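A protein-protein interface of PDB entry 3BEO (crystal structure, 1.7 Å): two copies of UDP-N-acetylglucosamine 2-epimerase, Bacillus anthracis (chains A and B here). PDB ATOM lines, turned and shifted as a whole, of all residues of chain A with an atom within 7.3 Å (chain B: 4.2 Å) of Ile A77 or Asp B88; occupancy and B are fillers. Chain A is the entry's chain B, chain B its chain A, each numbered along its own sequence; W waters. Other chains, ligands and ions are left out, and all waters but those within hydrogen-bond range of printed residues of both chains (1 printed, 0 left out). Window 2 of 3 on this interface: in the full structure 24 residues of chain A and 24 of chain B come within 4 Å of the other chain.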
ATOM      1  N   GLN A  74     -10.490  16.063  -6.114  1.00  0.00           N
ATOM      2  CA  GLN A  74     -11.011  16.512  -4.855  1.00  0.00           C
ATOM      3  C   GLN A  74     -12.525  16.369  -4.845  1.00  0.00           C
ATOM      4  O   GLN A  74     -13.199  16.410  -5.898  1.00  0.00           O
ATOM      5  CB  GLN A  74     -10.579  17.976  -4.595  1.00  0.00           C
ATOM      6  CG  GLN A  74     -11.228  19.025  -5.451  1.00  0.00           C
ATOM      7  CD  GLN A  74     -10.462  20.344  -5.482  1.00  0.00           C
ATOM      8  OE1 GLN A  74      -9.500  20.531  -4.735  1.00  0.00           O
ATOM      9  NE2 GLN A  74     -10.906  21.288  -6.343  1.00  0.00           N
ATOM     10  N   THR A  75     -13.051  16.245  -3.627  1.00  0.00           N
ATOM     11  CA  THR A  75     -14.483  16.144  -3.372  1.00  0.00           C
ATOM     12  C   THR A  75     -15.080  17.543  -3.039  1.00  0.00           C
ATOM     13  O   THR A  75     -14.374  18.505  -2.747  1.00  0.00           O
ATOM     14  CB  THR A  75     -14.742  15.176  -2.187  1.00  0.00           C
ATOM     15  OG1 THR A  75     -14.154  15.774  -1.014  1.00  0.00           O
ATOM     16  CG2 THR A  75     -14.115  13.734  -2.461  1.00  0.00           C
ATOM     17  N   LEU A  76     -16.395  17.642  -3.056  1.00  0.00           N
ATOM     18  CA  LEU A  76     -17.039  18.876  -2.634  1.00  0.00           C
ATOM     19  C   LEU A  76     -16.762  19.159  -1.160  1.00  0.00           C
ATOM     20  O   LEU A  76     -16.706  20.330  -0.738  1.00  0.00           O
ATOM     21  CB  LEU A  76     -18.532  18.802  -2.903  1.00  0.00           C
ATOM     22  CG  LEU A  76     -18.926  18.750  -4.389  1.00  0.00           C
ATOM     23  CD1 LEU A  76     -20.436  18.608  -4.545  1.00  0.00           C
ATOM     24  CD2 LEU A  76     -18.451  19.995  -5.116  1.00  0.00           C
ATOM     25  N   ILE A  77     -16.638  18.082  -0.361  1.00  0.00           N
ATOM     26  CA  ILE A  77     -16.314  18.236   1.070  1.00  0.00           C
ATOM     27  C   ILE A  77     -14.874  18.766   1.258  1.00  0.00           C
ATOM     28  O   ILE A  77     -14.654  19.612   2.069  1.00  0.00           O
ATOM     29  CB  ILE A  77     -16.568  17.004   1.852  1.00  0.00           C
ATOM     30  CG1 ILE A  77     -18.077  16.773   1.878  1.00  0.00           C
ATOM     31  CG2 ILE A  77     -16.084  17.144   3.380  1.00  0.00           C
ATOM     32  CD1 ILE A  77     -18.483  15.513   2.339  1.00  0.00           C
ATOM     33  N   ASP A  78     -13.930  18.282   0.454  1.00  0.00           N
ATOM     34  CA  ASP A  78     -12.547  18.800   0.420  1.00  0.00           C
ATOM     35  C   ASP A  78     -12.544  20.318   0.230  1.00  0.00           C
ATOM     36  O   ASP A  78     -11.954  21.063   1.052  1.00  0.00           O
ATOM     37  CB  ASP A  78     -11.726  18.178  -0.727  1.00  0.00           C
ATOM     38  CG  ASP A  78     -11.257  16.779  -0.460  1.00  0.00           C
ATOM     39  OD1 ASP A  78     -11.079  16.407   0.739  1.00  0.00           O
ATOM     40  OD2 ASP A  78     -11.053  16.056  -1.489  1.00  0.00           O
ATOM     41  N   ILE A  79     -13.270  20.775  -0.775  1.00  0.00           N
ATOM     42  CA  ILE A  79     -13.281  22.200  -1.103  1.00  0.00           C
ATOM     43  C   ILE A  79     -13.935  22.985   0.028  1.00  0.00           C
ATOM     44  O   ILE A  79     -13.411  23.958   0.551  1.00  0.00           O
ATOM     45  CB  ILE A  79     -14.032  22.506  -2.356  1.00  0.00           C
ATOM     46  CG1 ILE A  79     -13.405  21.736  -3.547  1.00  0.00           C
ATOM     47  CG2 ILE A  79     -14.034  24.001  -2.499  1.00  0.00           C
ATOM     48  CD1 ILE A  79     -14.354  21.637  -4.761  1.00  0.00           C
ATOM     49  N   THR A  80     -15.076  22.488   0.443  1.00  0.00           N
ATOM     50  CA  THR A  80     -15.864  23.160   1.446  1.00  0.00           C
ATOM     51  C   THR A  80     -15.101  23.350   2.765  1.00  0.00           C
ATOM     52  O   THR A  80     -15.142  24.430   3.332  1.00  0.00           O
ATOM     53  CB  THR A  80     -17.176  22.407   1.714  1.00  0.00           C
ATOM     54  OG1 THR A  80     -17.943  22.310   0.504  1.00  0.00           O
ATOM     55  CG2 THR A  80     -18.018  23.125   2.728  1.00  0.00           C
ATOM     56  N   THR A  81     -14.457  22.312   3.269  1.00  0.00           N
ATOM     57  CA  THR A  81     -13.768  22.439   4.580  1.00  0.00           C
ATOM     58  C   THR A  81     -12.457  23.242   4.457  1.00  0.00           C
ATOM     59  O   THR A  81     -12.175  24.143   5.268  1.00  0.00           O
ATOM     60  CB  THR A  81     -13.517  21.081   5.211  1.00  0.00           C
ATOM     61  OG1 THR A  81     -12.743  20.279   4.316  1.00  0.00           O
ATOM     62  CG2 THR A  81     -14.831  20.335   5.453  1.00  0.00           C
ATOM     63  N   ARG A  82     -11.658  22.955   3.420  1.00  0.00           N
ATOM     64  CA  ARG A  82     -10.347  23.614   3.269  1.00  0.00           C
ATOM     65  C   ARG A  82     -10.562  25.092   2.952  1.00  0.00           C
ATOM     66  O   ARG A  82      -9.843  25.950   3.438  1.00  0.00           O
ATOM     67  CB  ARG A  82      -9.518  22.949   2.168  1.00  0.00           C
ATOM     68  CG  ARG A  82      -9.126  21.508   2.466  1.00  0.00           C
ATOM     69  CD  ARG A  82      -8.840  20.751   1.261  1.00  0.00           C
ATOM     70  NE  ARG A  82      -7.553  21.076   0.664  1.00  0.00           N
ATOM     71  CZ  ARG A  82      -6.395  20.508   1.002  1.00  0.00           C
ATOM     72  NH1 ARG A  82      -6.332  19.639   1.998  1.00  0.00           N
ATOM     73  NH2 ARG A  82      -5.275  20.837   0.342  1.00  0.00           N
ATOM     74  N   GLY A  83     -11.550  25.385   2.130  1.00  0.00           N
ATOM     75  CA  GLY A  83     -11.933  26.715   1.793  1.00  0.00           C
ATOM     76  C   GLY A  83     -12.487  27.480   2.968  1.00  0.00           C
ATOM     77  O   GLY A  83     -12.053  28.608   3.249  1.00  0.00           O
ATOM     78  N   THR A 106     -18.312  26.178  -5.598  1.00  0.00           N
ATOM     79  CA  THR A 106     -18.233  25.881  -4.170  1.00  0.00           C
ATOM     80  C   THR A 106     -17.456  26.956  -3.395  1.00  0.00           C
ATOM     81  O   THR A 106     -17.864  27.344  -2.296  1.00  0.00           O
ATOM     82  CB  THR A 106     -17.771  24.429  -3.899  1.00  0.00           C
ATOM     83  OG1 THR A 106     -18.678  23.511  -4.525  1.00  0.00           O
ATOM     84  CG2 THR A 106     -17.685  24.182  -2.396  1.00  0.00           C
ATOM     85  N   LEU B  84     -19.956  18.195   9.056  1.00  0.00           N
ATOM     86  CA  LEU B  84     -20.033  17.809   7.642  1.00  0.00           C
ATOM     87  C   LEU B  84     -19.219  16.545   7.342  1.00  0.00           C
ATOM     88  O   LEU B  84     -19.674  15.648   6.617  1.00  0.00           O
ATOM     89  CB  LEU B  84     -19.544  18.973   6.762  1.00  0.00           C
ATOM     90  CG  LEU B  84     -19.581  18.692   5.254  1.00  0.00           C
ATOM     91  CD1 LEU B  84     -20.965  18.342   4.751  1.00  0.00           C
ATOM     92  CD2 LEU B  84     -19.062  19.983   4.560  1.00  0.00           C
ATOM     93  N   GLU B  85     -17.959  16.517   7.772  1.00  0.00           N
ATOM     94  CA  GLU B  85     -17.113  15.342   7.441  1.00  0.00           C
ATOM     95  C   GLU B  85     -17.710  14.066   8.032  1.00  0.00           C
ATOM     96  O   GLU B  85     -17.753  13.054   7.372  1.00  0.00           O
ATOM     97  CB  GLU B  85     -15.698  15.503   7.919  1.00  0.00           C
ATOM     98  CG  GLU B  85     -14.947  16.560   7.243  1.00  0.00           C
ATOM     99  CD  GLU B  85     -13.626  16.865   7.900  1.00  0.00           C
ATOM    100  OE1 GLU B  85     -13.461  16.594   9.117  1.00  0.00           O
ATOM    101  OE2 GLU B  85     -12.736  17.405   7.188  1.00  0.00           O
ATOM    102  N   GLY B  86     -18.188  14.131   9.278  1.00  0.00           N
ATOM    103  CA  GLY B  86     -18.719  12.950   9.917  1.00  0.00           C
ATOM    104  C   GLY B  86     -20.037  12.474   9.329  1.00  0.00           C
ATOM    105  O   GLY B  86     -20.259  11.286   9.137  1.00  0.00           O
ATOM    106  N   LEU B  87     -20.912  13.422   9.021  1.00  0.00           N
ATOM    107  CA  LEU B  87     -22.219  13.080   8.460  1.00  0.00           C
ATOM    108  C   LEU B  87     -22.038  12.513   7.038  1.00  0.00           C
ATOM    109  O   LEU B  87     -22.763  11.630   6.642  1.00  0.00           O
ATOM    110  CB  LEU B  87     -23.172  14.284   8.466  1.00  0.00           C
ATOM    111  CG  LEU B  87     -23.682  14.637   9.886  1.00  0.00           C
ATOM    112  CD1 LEU B  87     -24.701  15.779   9.828  1.00  0.00           C
ATOM    113  CD2 LEU B  87     -24.330  13.394  10.648  1.00  0.00           C
ATOM    114  N   ASP B  88     -21.057  13.013   6.293  1.00  0.00           N
ATOM    115  CA  ASP B  88     -20.843  12.482   4.924  1.00  0.00           C
ATOM    116  C   ASP B  88     -20.489  11.004   5.035  1.00  0.00           C
ATOM    117  O   ASP B  88     -20.976  10.132   4.304  1.00  0.00           O
ATOM    118  CB  ASP B  88     -19.733  13.272   4.252  1.00  0.00           C
ATOM    119  CG  ASP B  88     -19.359  12.727   2.930  1.00  0.00           C
ATOM    120  OD1 ASP B  88     -20.246  12.706   2.055  1.00  0.00           O
ATOM    121  OD2 ASP B  88     -18.150  12.341   2.773  1.00  0.00           O
ATOM    122  N   LYS B  89     -19.631  10.688   5.993  1.00  0.00           N
ATOM    123  CA  LYS B  89     -19.258   9.290   6.223  1.00  0.00           C
ATOM    124  C   LYS B  89     -20.478   8.443   6.588  1.00  0.00           C
ATOM    125  O   LYS B  89     -20.614   7.332   6.080  1.00  0.00           O
ATOM    126  CB  LYS B  89     -18.165   9.223   7.263  1.00  0.00           C
ATOM    127  CG  LYS B  89     -16.917   9.891   6.771  1.00  0.00           C
ATOM    128  CD  LYS B  89     -15.780   9.795   7.702  1.00  0.00           C
ATOM    129  CE  LYS B  89     -14.616  10.681   7.230  1.00  0.00           C
ATOM    130  NZ  LYS B  89     -13.293  10.286   7.814  1.00  0.00           N
ATOM    131  N   VAL B  90     -21.332   8.966   7.497  1.00  0.00           N
ATOM    132  CA  VAL B  90     -22.515   8.185   7.973  1.00  0.00           C
ATOM    133  C   VAL B  90     -23.443   7.920   6.786  1.00  0.00           C
ATOM    134  O   VAL B  90     -24.030   6.804   6.649  1.00  0.00           O
ATOM    135  CB  VAL B  90     -23.240   8.921   9.148  1.00  0.00           C
ATOM    136  CG1 VAL B  90     -24.623   8.321   9.427  1.00  0.00           C
ATOM    137  CG2 VAL B  90     -22.385   8.834  10.427  1.00  0.00           C
ATOM    138  N   MET B  91     -23.622   8.938   5.958  1.00  0.00           N
ATOM    139  CA  MET B  91     -24.554   8.847   4.827  1.00  0.00           C
ATOM    140  C   MET B  91     -24.089   7.899   3.756  1.00  0.00           C
ATOM    141  O   MET B  91     -24.911   7.187   3.173  1.00  0.00           O
ATOM    142  CB  MET B  91     -24.867  10.225   4.244  1.00  0.00           C
ATOM    143  CG  MET B  91     -25.735  11.080   5.190  1.00  0.00           C
ATOM    144  SD  MET B  91     -25.984  12.713   4.564  1.00  0.00           S
ATOM    145  CE  MET B  91     -26.633  13.477   6.062  1.00  0.00           C
ATOM    146  N   LYS B  92     -22.777   7.844   3.555  1.00  0.00           N
ATOM    147  CA  LYS B  92     -22.168   6.896   2.590  1.00  0.00           C
ATOM    148  C   LYS B  92     -22.269   5.450   3.066  1.00  0.00           C
ATOM    149  O   LYS B  92     -22.395   4.528   2.230  1.00  0.00           O
ATOM    150  CB  LYS B  92     -20.718   7.324   2.304  1.00  0.00           C
ATOM    151  CG  LYS B  92     -20.621   8.411   1.276  1.00  0.00           C
ATOM    152  CD  LYS B  92     -19.212   8.907   1.075  1.00  0.00           C
ATOM    153  CE  LYS B  92     -19.098   9.795  -0.115  1.00  0.00           C
ATOM    154  NZ  LYS B  92     -19.850  11.109  -0.037  1.00  0.00           N
ATOM    155  N   TYR B 117     -24.911  16.870  -0.752  1.00  0.00           N
ATOM    156  CA  TYR B 117     -23.656  16.334  -1.243  1.00  0.00           C
ATOM    157  C   TYR B 117     -23.639  14.821  -1.554  1.00  0.00           C
ATOM    158  O   TYR B 117     -22.704  14.355  -2.201  1.00  0.00           O
ATOM    159  CB  TYR B 117     -22.485  16.678  -0.304  1.00  0.00           C
ATOM    160  CG  TYR B 117     -22.001  18.125  -0.336  1.00  0.00           C
ATOM    161  CD1 TYR B 117     -22.472  19.041  -1.254  1.00  0.00           C
ATOM    162  CD2 TYR B 117     -21.024  18.549   0.535  1.00  0.00           C
ATOM    163  CE1 TYR B 117     -21.951  20.353  -1.309  1.00  0.00           C
ATOM    164  CE2 TYR B 117     -20.551  19.844   0.512  1.00  0.00           C
ATOM    165  CZ  TYR B 117     -21.015  20.736  -0.407  1.00  0.00           C
ATOM    166  OH  TYR B 117     -20.532  22.039  -0.435  1.00  0.00           O
ATOM    167  N   ASN B 118     -24.689  14.106  -1.152  1.00  0.00           N
ATOM    168  CA  ASN B 118     -24.886  12.687  -1.429  1.00  0.00           C
ATOM    169  C   ASN B 118     -26.171  12.450  -2.272  1.00  0.00           C
ATOM    170  O   ASN B 118     -26.577  11.326  -2.477  1.00  0.00           O
ATOM    171  CB  ASN B 118     -24.901  11.926  -0.106  1.00  0.00           C
ATOM    172  CG  ASN B 118     -23.518  11.759   0.462  1.00  0.00           C
ATOM    173  OD1 ASN B 118     -22.756  10.887   0.026  1.00  0.00           O
ATOM    174  ND2 ASN B 118     -23.215  12.527   1.485  1.00  0.00           N
HETATM  175  O   HOH W   1     -21.002  23.226  -2.915  1.00  0.00           O
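No position is printed for both chains.
Of the 6 pairs that touch across the chains among the printed residues, none has its exchanged pair printed and touching as well.
Water W1 bridges the side-chain hydroxyl (OH) of Tyr B117 (2.8 Å) and the side-chain hydroxyl (OG1) of Thr A106 (2.8 Å).
OH of Tyr B117 is in hydrogen-bond range of OG1 of Thr A80 (2.8 Å).
Of chain B, only Asp B88 (3.0 Å) and Tyr B117 (3.7 Å) come within 4 Å of Ile A77.
Of chain A, only Ile A77 (3.0 Å) comes within 4 Å of Asp B88.
Printed residues of chain B within 4 Å of Thr A81: Glu B85 (3.998 Å).
Of the printed residues of chain B, Thr A80 touches Leu B84 (3.8 Å) and Tyr B117 (2.8 Å).
Leu B87 touches none of the printed residues of chain A.
Along chain B the printed residues that touch a printed residue of chain A span positions 84 to 117.
Among the printed residues, no Asp or Glu carboxylate lies within 4 Å of a Lys or Arg side-chain nitrogen of the other chain.
The side-chain hydroxyl of Thr A75 sits close to the backbone NH of Ile A77.
NZ of Lys B92 lies within salt-bridge range of OD1 of Asp B88.
The backbone carbonyl oxygen (O) of Leu A76 lies within hydrogen-bond range of the side-chain hydroxyl (OG1) of Thr A80 (2.6 Å).
The side-chain carboxylate of Asp B88 is in hydrogen-bond range of the side-chain amide nitrogen of Asn B118 (3.0 Å).
The side-chain hydroxyl (OG1) of Thr A81 lies within hydrogen-bond range of the backbone carbonyl oxygen (O) of Ile A77 (3.0 Å).
O of Asp A78 sits at hydrogen-bond distance from OG1 of Thr A81, 3.4 Å away.
Among the printed residues, pairs that only touch across the chains: Ile A77 with Asp B88 (3.0 Å), Ile A77 with Tyr B117 (3.7 Å), Thr A80 with Leu B84 (3.8 Å), Leu A76 with Tyr B117 (3.9 Å) and Thr A81 with Glu B85 (3.998 Å).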
